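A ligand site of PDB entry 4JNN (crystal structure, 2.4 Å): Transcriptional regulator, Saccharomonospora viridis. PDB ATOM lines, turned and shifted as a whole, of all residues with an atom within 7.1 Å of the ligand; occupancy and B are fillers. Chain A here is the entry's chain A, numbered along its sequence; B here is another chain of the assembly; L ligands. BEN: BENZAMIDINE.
Trp 98 touches the ligand. Trp 101 touches the ligand (CZ2 to C5, 3.8 Å). Ala 121 touches the ligand (O to C4, 3.9 Å). CD1 of Tyr 122 touches N2 of the ligand, at 3.999 Å. CE3 of Trp 125 touches C2 of the ligand (3.5 Å). Hydrophobic or aromatic side chains within 4 Å of the ligand: Trp 98, Trp 101, Tyr 118, Tyr 122 and Trp 125. Of the 20 residues printed, 8 come within 4 Å of the ligand. The nearest printed residue that does not touch the ligand is Trp 105 (4.7 Å).
NE1 of Trp 105 is in hydrogen-bond range of OH of Tyr 118 (3.2 Å). The backbone carbonyl oxygen (O) of Gln 87 sits at hydrogen-bond distance from the indole nitrogen (NE1) of Trp 98, 2.8 Å away. The side-chain hydroxyl (OG) of Ser 155 lies within hydrogen-bond range of the side-chain hydroxyl (OH) of Tyr 122 (3.1 Å).
OE1 of Gln 87 lies within hydrogen-bond range of N1 of the ligand. A nitrogen (N2) of the ligand lies within hydrogen-bond range of the side-chain hydroxyl (OH) of Tyr 118. N2 of the ligand lies within salt-bridge range of OD1 of Asp 159 (2.7 Å).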
ATOM      1  N   LEU A  55     -25.581  -9.100   3.949  1.00  0.00           N
ATOM      2  CA  LEU A  55     -25.413 -10.389   3.307  1.00  0.00           C
ATOM      3  C   LEU A  55     -26.717 -11.016   2.721  1.00  0.00           C
ATOM      4  O   LEU A  55     -26.737 -11.507   1.597  1.00  0.00           O
ATOM      5  CB  LEU A  55     -24.788 -11.314   4.338  1.00  0.00           C
ATOM      6  CG  LEU A  55     -24.727 -12.800   4.112  1.00  0.00           C
ATOM      7  CD1 LEU A  55     -23.907 -13.129   2.885  1.00  0.00           C
ATOM      8  CD2 LEU A  55     -24.176 -13.499   5.365  1.00  0.00           C
ATOM      9  N   VAL A  59     -27.015 -11.751  -1.354  1.00  0.00           N
ATOM     10  CA  VAL A  59     -27.494 -13.057  -1.783  1.00  0.00           C
ATOM     11  C   VAL A  59     -28.822 -13.030  -2.539  1.00  0.00           C
ATOM     12  O   VAL A  59     -29.040 -13.852  -3.415  1.00  0.00           O
ATOM     13  CB  VAL A  59     -27.615 -13.981  -0.578  1.00  0.00           C
ATOM     14  CG1 VAL A  59     -28.667 -15.076  -0.800  1.00  0.00           C
ATOM     15  CG2 VAL A  59     -26.247 -14.533  -0.301  1.00  0.00           C
ATOM     16  N   ALA A  62     -27.619 -11.371  -5.999  1.00  0.00           N
ATOM     17  CA  ALA A  62     -26.776 -12.246  -6.829  1.00  0.00           C
ATOM     18  C   ALA A  62     -27.613 -13.302  -7.546  1.00  0.00           C
ATOM     19  O   ALA A  62     -27.397 -13.565  -8.734  1.00  0.00           O
ATOM     20  CB  ALA A  62     -25.621 -12.902  -6.023  1.00  0.00           C
ATOM     21  N   GLN A  66     -28.432 -13.908 -11.429  1.00  0.00           N
ATOM     22  CA  GLN A  66     -28.284 -15.191 -12.050  1.00  0.00           C
ATOM     23  C   GLN A  66     -29.505 -15.676 -12.864  1.00  0.00           C
ATOM     24  O   GLN A  66     -29.335 -16.162 -13.981  1.00  0.00           O
ATOM     25  CB  GLN A  66     -27.856 -16.228 -11.035  1.00  0.00           C
ATOM     26  CG  GLN A  66     -28.129 -17.641 -11.503  1.00  0.00           C
ATOM     27  CD  GLN A  66     -27.988 -18.619 -10.340  1.00  0.00           C
ATOM     28  OE1 GLN A  66     -26.960 -18.619  -9.615  1.00  0.00           O
ATOM     29  NE2 GLN A  66     -29.021 -19.440 -10.145  1.00  0.00           N
ATOM     30  N   GLN A  87     -19.591 -16.236 -11.542  1.00  0.00           N
ATOM     31  CA  GLN A  87     -18.802 -16.488 -10.341  1.00  0.00           C
ATOM     32  C   GLN A  87     -17.417 -15.886 -10.376  1.00  0.00           C
ATOM     33  O   GLN A  87     -16.663 -16.020  -9.428  1.00  0.00           O
ATOM     34  CB  GLN A  87     -18.615 -17.981 -10.110  1.00  0.00           C
ATOM     35  CG  GLN A  87     -19.769 -18.662  -9.391  1.00  0.00           C
ATOM     36  CD  GLN A  87     -20.281 -17.892  -8.178  1.00  0.00           C
ATOM     37  OE1 GLN A  87     -19.557 -17.716  -7.182  1.00  0.00           O
ATOM     38  NE2 GLN A  87     -21.533 -17.440  -8.242  1.00  0.00           N
ATOM     39  N   TRP A  98     -17.132 -11.449  -3.650  1.00  0.00           N
ATOM     40  CA  TRP A  98     -16.097 -12.412  -3.195  1.00  0.00           C
ATOM     41  C   TRP A  98     -15.461 -11.999  -1.863  1.00  0.00           C
ATOM     42  O   TRP A  98     -15.104 -12.807  -1.029  1.00  0.00           O
ATOM     43  CB  TRP A  98     -15.045 -12.617  -4.278  1.00  0.00           C
ATOM     44  CG  TRP A  98     -15.493 -13.661  -5.273  1.00  0.00           C
ATOM     45  CD1 TRP A  98     -16.253 -13.467  -6.417  1.00  0.00           C
ATOM     46  CD2 TRP A  98     -15.284 -15.086  -5.187  1.00  0.00           C
ATOM     47  NE1 TRP A  98     -16.509 -14.670  -7.027  1.00  0.00           N
ATOM     48  CE2 TRP A  98     -15.881 -15.673  -6.310  1.00  0.00           C
ATOM     49  CE3 TRP A  98     -14.619 -15.916  -4.260  1.00  0.00           C
ATOM     50  CZ2 TRP A  98     -15.844 -17.039  -6.540  1.00  0.00           C
ATOM     51  CZ3 TRP A  98     -14.581 -17.275  -4.482  1.00  0.00           C
ATOM     52  CH2 TRP A  98     -15.200 -17.820  -5.605  1.00  0.00           C
ATOM     53  N   TRP A 101     -17.729 -13.037   0.858  1.00  0.00           N
ATOM     54  CA  TRP A 101     -17.719 -14.518   0.957  1.00  0.00           C
ATOM     55  C   TRP A 101     -16.595 -14.922   1.866  1.00  0.00           C
ATOM     56  O   TRP A 101     -16.823 -15.694   2.810  1.00  0.00           O
ATOM     57  CB  TRP A 101     -17.554 -15.245  -0.400  1.00  0.00           C
ATOM     58  CG  TRP A 101     -18.681 -14.994  -1.385  1.00  0.00           C
ATOM     59  CD1 TRP A 101     -18.569 -14.924  -2.760  1.00  0.00           C
ATOM     60  CD2 TRP A 101     -20.040 -14.745  -1.082  1.00  0.00           C
ATOM     61  NE1 TRP A 101     -19.800 -14.650  -3.329  1.00  0.00           N
ATOM     62  CE2 TRP A 101     -20.717 -14.539  -2.315  1.00  0.00           C
ATOM     63  CE3 TRP A 101     -20.770 -14.675   0.107  1.00  0.00           C
ATOM     64  CZ2 TRP A 101     -22.085 -14.253  -2.379  1.00  0.00           C
ATOM     65  CZ3 TRP A 101     -22.137 -14.410   0.050  1.00  0.00           C
ATOM     66  CH2 TRP A 101     -22.785 -14.203  -1.183  1.00  0.00           C
ATOM     67  N   TRP A 105     -17.068 -16.892   5.321  1.00  0.00           N
ATOM     68  CA  TRP A 105     -16.559 -18.208   5.652  1.00  0.00           C
ATOM     69  C   TRP A 105     -15.951 -18.293   7.056  1.00  0.00           C
ATOM     70  O   TRP A 105     -16.154 -19.313   7.754  1.00  0.00           O
ATOM     71  CB  TRP A 105     -15.543 -18.692   4.667  1.00  0.00           C
ATOM     72  CG  TRP A 105     -15.966 -18.800   3.278  1.00  0.00           C
ATOM     73  CD1 TRP A 105     -17.235 -19.032   2.801  1.00  0.00           C
ATOM     74  CD2 TRP A 105     -15.111 -18.691   2.133  1.00  0.00           C
ATOM     75  NE1 TRP A 105     -17.199 -19.105   1.421  1.00  0.00           N
ATOM     76  CE2 TRP A 105     -15.900 -18.893   0.992  1.00  0.00           C
ATOM     77  CE3 TRP A 105     -13.741 -18.490   1.968  1.00  0.00           C
ATOM     78  CZ2 TRP A 105     -15.380 -18.833  -0.306  1.00  0.00           C
ATOM     79  CZ3 TRP A 105     -13.211 -18.452   0.705  1.00  0.00           C
ATOM     80  CH2 TRP A 105     -14.030 -18.634  -0.429  1.00  0.00           C
ATOM     81  N   TYR A 118     -25.520 -18.565   5.108  1.00  0.00           N
ATOM     82  CA  TYR A 118     -24.547 -18.850   4.042  1.00  0.00           C
ATOM     83  C   TYR A 118     -24.776 -20.236   3.414  1.00  0.00           C
ATOM     84  O   TYR A 118     -24.644 -20.396   2.233  1.00  0.00           O
ATOM     85  CB  TYR A 118     -23.093 -18.724   4.480  1.00  0.00           C
ATOM     86  CG  TYR A 118     -22.161 -19.273   3.399  1.00  0.00           C
ATOM     87  CD1 TYR A 118     -21.790 -18.465   2.305  1.00  0.00           C
ATOM     88  CD2 TYR A 118     -21.713 -20.597   3.416  1.00  0.00           C
ATOM     89  CE1 TYR A 118     -20.992 -18.961   1.277  1.00  0.00           C
ATOM     90  CE2 TYR A 118     -20.894 -21.093   2.389  1.00  0.00           C
ATOM     91  CZ  TYR A 118     -20.544 -20.280   1.330  1.00  0.00           C
ATOM     92  OH  TYR A 118     -19.737 -20.726   0.297  1.00  0.00           O
ATOM     93  N   ASP A 120     -27.711 -21.889   3.113  1.00  0.00           N
ATOM     94  CA  ASP A 120     -28.874 -21.846   2.214  1.00  0.00           C
ATOM     95  C   ASP A 120     -28.469 -21.287   0.917  1.00  0.00           C
ATOM     96  O   ASP A 120     -28.891 -21.800  -0.114  1.00  0.00           O
ATOM     97  CB  ASP A 120     -29.999 -20.959   2.766  1.00  0.00           C
ATOM     98  CG  ASP A 120     -30.678 -21.608   3.940  1.00  0.00           C
ATOM     99  OD1 ASP A 120     -30.398 -22.822   4.131  1.00  0.00           O
ATOM    100  OD2 ASP A 120     -31.472 -20.928   4.667  1.00  0.00           O
ATOM    101  N   ALA A 121     -27.670 -20.231   0.939  1.00  0.00           N
ATOM    102  CA  ALA A 121     -27.380 -19.535  -0.316  1.00  0.00           C
ATOM    103  C   ALA A 121     -26.467 -20.407  -1.158  1.00  0.00           C
ATOM    104  O   ALA A 121     -26.644 -20.547  -2.377  1.00  0.00           O
ATOM    105  CB  ALA A 121     -26.747 -18.170  -0.072  1.00  0.00           C
ATOM    106  N   TYR A 122     -25.489 -21.009  -0.498  1.00  0.00           N
ATOM    107  CA  TYR A 122     -24.580 -21.841  -1.254  1.00  0.00           C
ATOM    108  C   TYR A 122     -25.356 -23.054  -1.845  1.00  0.00           C
ATOM    109  O   TYR A 122     -25.279 -23.349  -3.039  1.00  0.00           O
ATOM    110  CB  TYR A 122     -23.394 -22.279  -0.364  1.00  0.00           C
ATOM    111  CG  TYR A 122     -22.600 -23.386  -1.017  1.00  0.00           C
ATOM    112  CD1 TYR A 122     -21.510 -23.136  -1.840  1.00  0.00           C
ATOM    113  CD2 TYR A 122     -23.007 -24.698  -0.842  1.00  0.00           C
ATOM    114  CE1 TYR A 122     -20.820 -24.170  -2.431  1.00  0.00           C
ATOM    115  CE2 TYR A 122     -22.358 -25.726  -1.427  1.00  0.00           C
ATOM    116  CZ  TYR A 122     -21.269 -25.484  -2.215  1.00  0.00           C
ATOM    117  OH  TYR A 122     -20.698 -26.629  -2.749  1.00  0.00           O
ATOM    118  N   ASP A 123     -26.115 -23.727  -0.972  1.00  0.00           N
ATOM    119  CA  ASP A 123     -26.921 -24.868  -1.315  1.00  0.00           C
ATOM    120  C   ASP A 123     -27.791 -24.641  -2.498  1.00  0.00           C
ATOM    121  O   ASP A 123     -27.918 -25.516  -3.344  1.00  0.00           O
ATOM    122  CB  ASP A 123     -27.817 -25.283  -0.157  1.00  0.00           C
ATOM    123  CG  ASP A 123     -28.063 -26.777  -0.145  1.00  0.00           C
ATOM    124  OD1 ASP A 123     -28.607 -27.294  -1.123  1.00  0.00           O
ATOM    125  OD2 ASP A 123     -27.685 -27.447   0.849  1.00  0.00           O
ATOM    126  N   ARG A 124     -28.394 -23.454  -2.573  1.00  0.00           N
ATOM    127  CA  ARG A 124     -29.230 -23.093  -3.673  1.00  0.00           C
ATOM    128  C   ARG A 124     -28.498 -23.039  -5.021  1.00  0.00           C
ATOM    129  O   ARG A 124     -29.055 -23.386  -6.066  1.00  0.00           O
ATOM    130  CB  ARG A 124     -29.830 -21.724  -3.382  1.00  0.00           C
ATOM    131  CG  ARG A 124     -30.661 -21.156  -4.527  1.00  0.00           C
ATOM    132  CD  ARG A 124     -31.285 -19.841  -4.061  1.00  0.00           C
ATOM    133  NE  ARG A 124     -32.625 -19.650  -4.601  1.00  0.00           N
ATOM    134  CZ  ARG A 124     -33.457 -18.679  -4.207  1.00  0.00           C
ATOM    135  NH1 ARG A 124     -33.062 -17.805  -3.261  1.00  0.00           N
ATOM    136  NH2 ARG A 124     -34.684 -18.576  -4.753  1.00  0.00           N
ATOM    137  N   TRP A 125     -27.262 -22.557  -4.992  1.00  0.00           N
ATOM    138  CA  TRP A 125     -26.461 -22.329  -6.158  1.00  0.00           C
ATOM    139  C   TRP A 125     -25.839 -23.674  -6.525  1.00  0.00           C
ATOM    140  O   TRP A 125     -25.820 -24.086  -7.666  1.00  0.00           O
ATOM    141  CB  TRP A 125     -25.412 -21.236  -5.837  1.00  0.00           C
ATOM    142  CG  TRP A 125     -24.333 -21.117  -6.826  1.00  0.00           C
ATOM    143  CD1 TRP A 125     -24.390 -20.530  -8.080  1.00  0.00           C
ATOM    144  CD2 TRP A 125     -23.011 -21.639  -6.677  1.00  0.00           C
ATOM    145  NE1 TRP A 125     -23.144 -20.669  -8.731  1.00  0.00           N
ATOM    146  CE2 TRP A 125     -22.291 -21.335  -7.879  1.00  0.00           C
ATOM    147  CE3 TRP A 125     -22.344 -22.309  -5.639  1.00  0.00           C
ATOM    148  CZ2 TRP A 125     -20.933 -21.707  -8.051  1.00  0.00           C
ATOM    149  CZ3 TRP A 125     -21.007 -22.660  -5.819  1.00  0.00           C
ATOM    150  CH2 TRP A 125     -20.317 -22.357  -7.007  1.00  0.00           C
ATOM    151  N   TYR A 126     -25.408 -24.420  -5.539  1.00  0.00           N
ATOM    152  CA  TYR A 126     -24.989 -25.760  -5.813  1.00  0.00           C
ATOM    153  C   TYR A 126     -26.072 -26.654  -6.491  1.00  0.00           C
ATOM    154  O   TYR A 126     -25.731 -27.393  -7.425  1.00  0.00           O
ATOM    155  CB  TYR A 126     -24.594 -26.359  -4.485  1.00  0.00           C
ATOM    156  CG  TYR A 126     -24.291 -27.808  -4.482  1.00  0.00           C
ATOM    157  CD1 TYR A 126     -23.052 -28.269  -4.936  1.00  0.00           C
ATOM    158  CD2 TYR A 126     -25.202 -28.718  -3.945  1.00  0.00           C
ATOM    159  CE1 TYR A 126     -22.753 -29.612  -4.909  1.00  0.00           C
ATOM    160  CE2 TYR A 126     -24.913 -30.061  -3.919  1.00  0.00           C
ATOM    161  CZ  TYR A 126     -23.665 -30.501  -4.379  1.00  0.00           C
ATOM    162  OH  TYR A 126     -23.316 -31.850  -4.330  1.00  0.00           O
ATOM    163  N   SER A 155     -17.768 -26.696  -7.917  1.00  0.00           N
ATOM    164  CA  SER A 155     -17.940 -25.583  -7.011  1.00  0.00           C
ATOM    165  C   SER A 155     -16.756 -25.415  -6.007  1.00  0.00           C
ATOM    166  O   SER A 155     -16.379 -24.300  -5.664  1.00  0.00           O
ATOM    167  CB  SER A 155     -19.238 -25.795  -6.278  1.00  0.00           C
ATOM    168  OG  SER A 155     -19.010 -26.772  -5.318  1.00  0.00           O
ATOM    169  N   ILE A 158     -14.086 -23.577  -8.222  1.00  0.00           N
ATOM    170  CA  ILE A 158     -14.384 -22.168  -8.367  1.00  0.00           C
ATOM    171  C   ILE A 158     -13.936 -21.383  -7.124  1.00  0.00           C
ATOM    172  O   ILE A 158     -13.322 -20.329  -7.249  1.00  0.00           O
ATOM    173  CB  ILE A 158     -15.904 -21.990  -8.544  1.00  0.00           C
ATOM    174  CG1 ILE A 158     -16.285 -22.464  -9.969  1.00  0.00           C
ATOM    175  CG2 ILE A 158     -16.290 -20.575  -8.133  1.00  0.00           C
ATOM    176  CD1 ILE A 158     -17.786 -22.523 -10.265  1.00  0.00           C
ATOM    177  N   ASP A 159     -14.268 -21.916  -5.944  1.00  0.00           N
ATOM    178  CA  ASP A 159     -13.856 -21.311  -4.671  1.00  0.00           C
ATOM    179  C   ASP A 159     -12.320 -21.296  -4.509  1.00  0.00           C
ATOM    180  O   ASP A 159     -11.742 -20.276  -4.134  1.00  0.00           O
ATOM    181  CB  ASP A 159     -14.532 -22.066  -3.493  1.00  0.00           C
ATOM    182  CG  ASP A 159     -16.015 -21.614  -3.252  1.00  0.00           C
ATOM    183  OD1 ASP A 159     -16.467 -20.581  -3.822  1.00  0.00           O
ATOM    184  OD2 ASP A 159     -16.729 -22.290  -2.499  1.00  0.00           O
ATOM    185  N   ILE B 163     -13.062 -25.393   2.728  1.00  0.00           N
ATOM    186  CA  ILE B 163     -14.130 -24.449   3.036  1.00  0.00           C
ATOM    187  C   ILE B 163     -15.467 -25.174   3.260  1.00  0.00           C
ATOM    188  O   ILE B 163     -16.177 -24.915   4.256  1.00  0.00           O
ATOM    189  CB  ILE B 163     -14.265 -23.372   1.890  1.00  0.00           C
ATOM    190  CG1 ILE B 163     -13.052 -22.430   1.880  1.00  0.00           C
ATOM    191  CG2 ILE B 163     -15.581 -22.578   1.939  1.00  0.00           C
ATOM    192  CD1 ILE B 163     -12.833 -21.881   0.471  1.00  0.00           C
HETATM  193  C1  BEN L   1     -20.962 -18.863  -3.517  1.00  0.00           C
HETATM  194  C2  BEN L   1     -21.875 -19.037  -4.541  1.00  0.00           C
HETATM  195  C3  BEN L   1     -23.193 -18.693  -4.312  1.00  0.00           C
HETATM  196  C4  BEN L   1     -23.608 -18.196  -3.081  1.00  0.00           C
HETATM  197  C5  BEN L   1     -22.685 -18.022  -2.043  1.00  0.00           C
HETATM  198  C6  BEN L   1     -21.366 -18.366  -2.272  1.00  0.00           C
HETATM  199  C   BEN L   1     -19.522 -19.239  -3.736  1.00  0.00           C
HETATM  200  N1  BEN L   1     -18.852 -18.661  -4.579  1.00  0.00           N
HETATM  201  N2  BEN L   1     -19.018 -20.218  -2.966  1.00  0.00           N
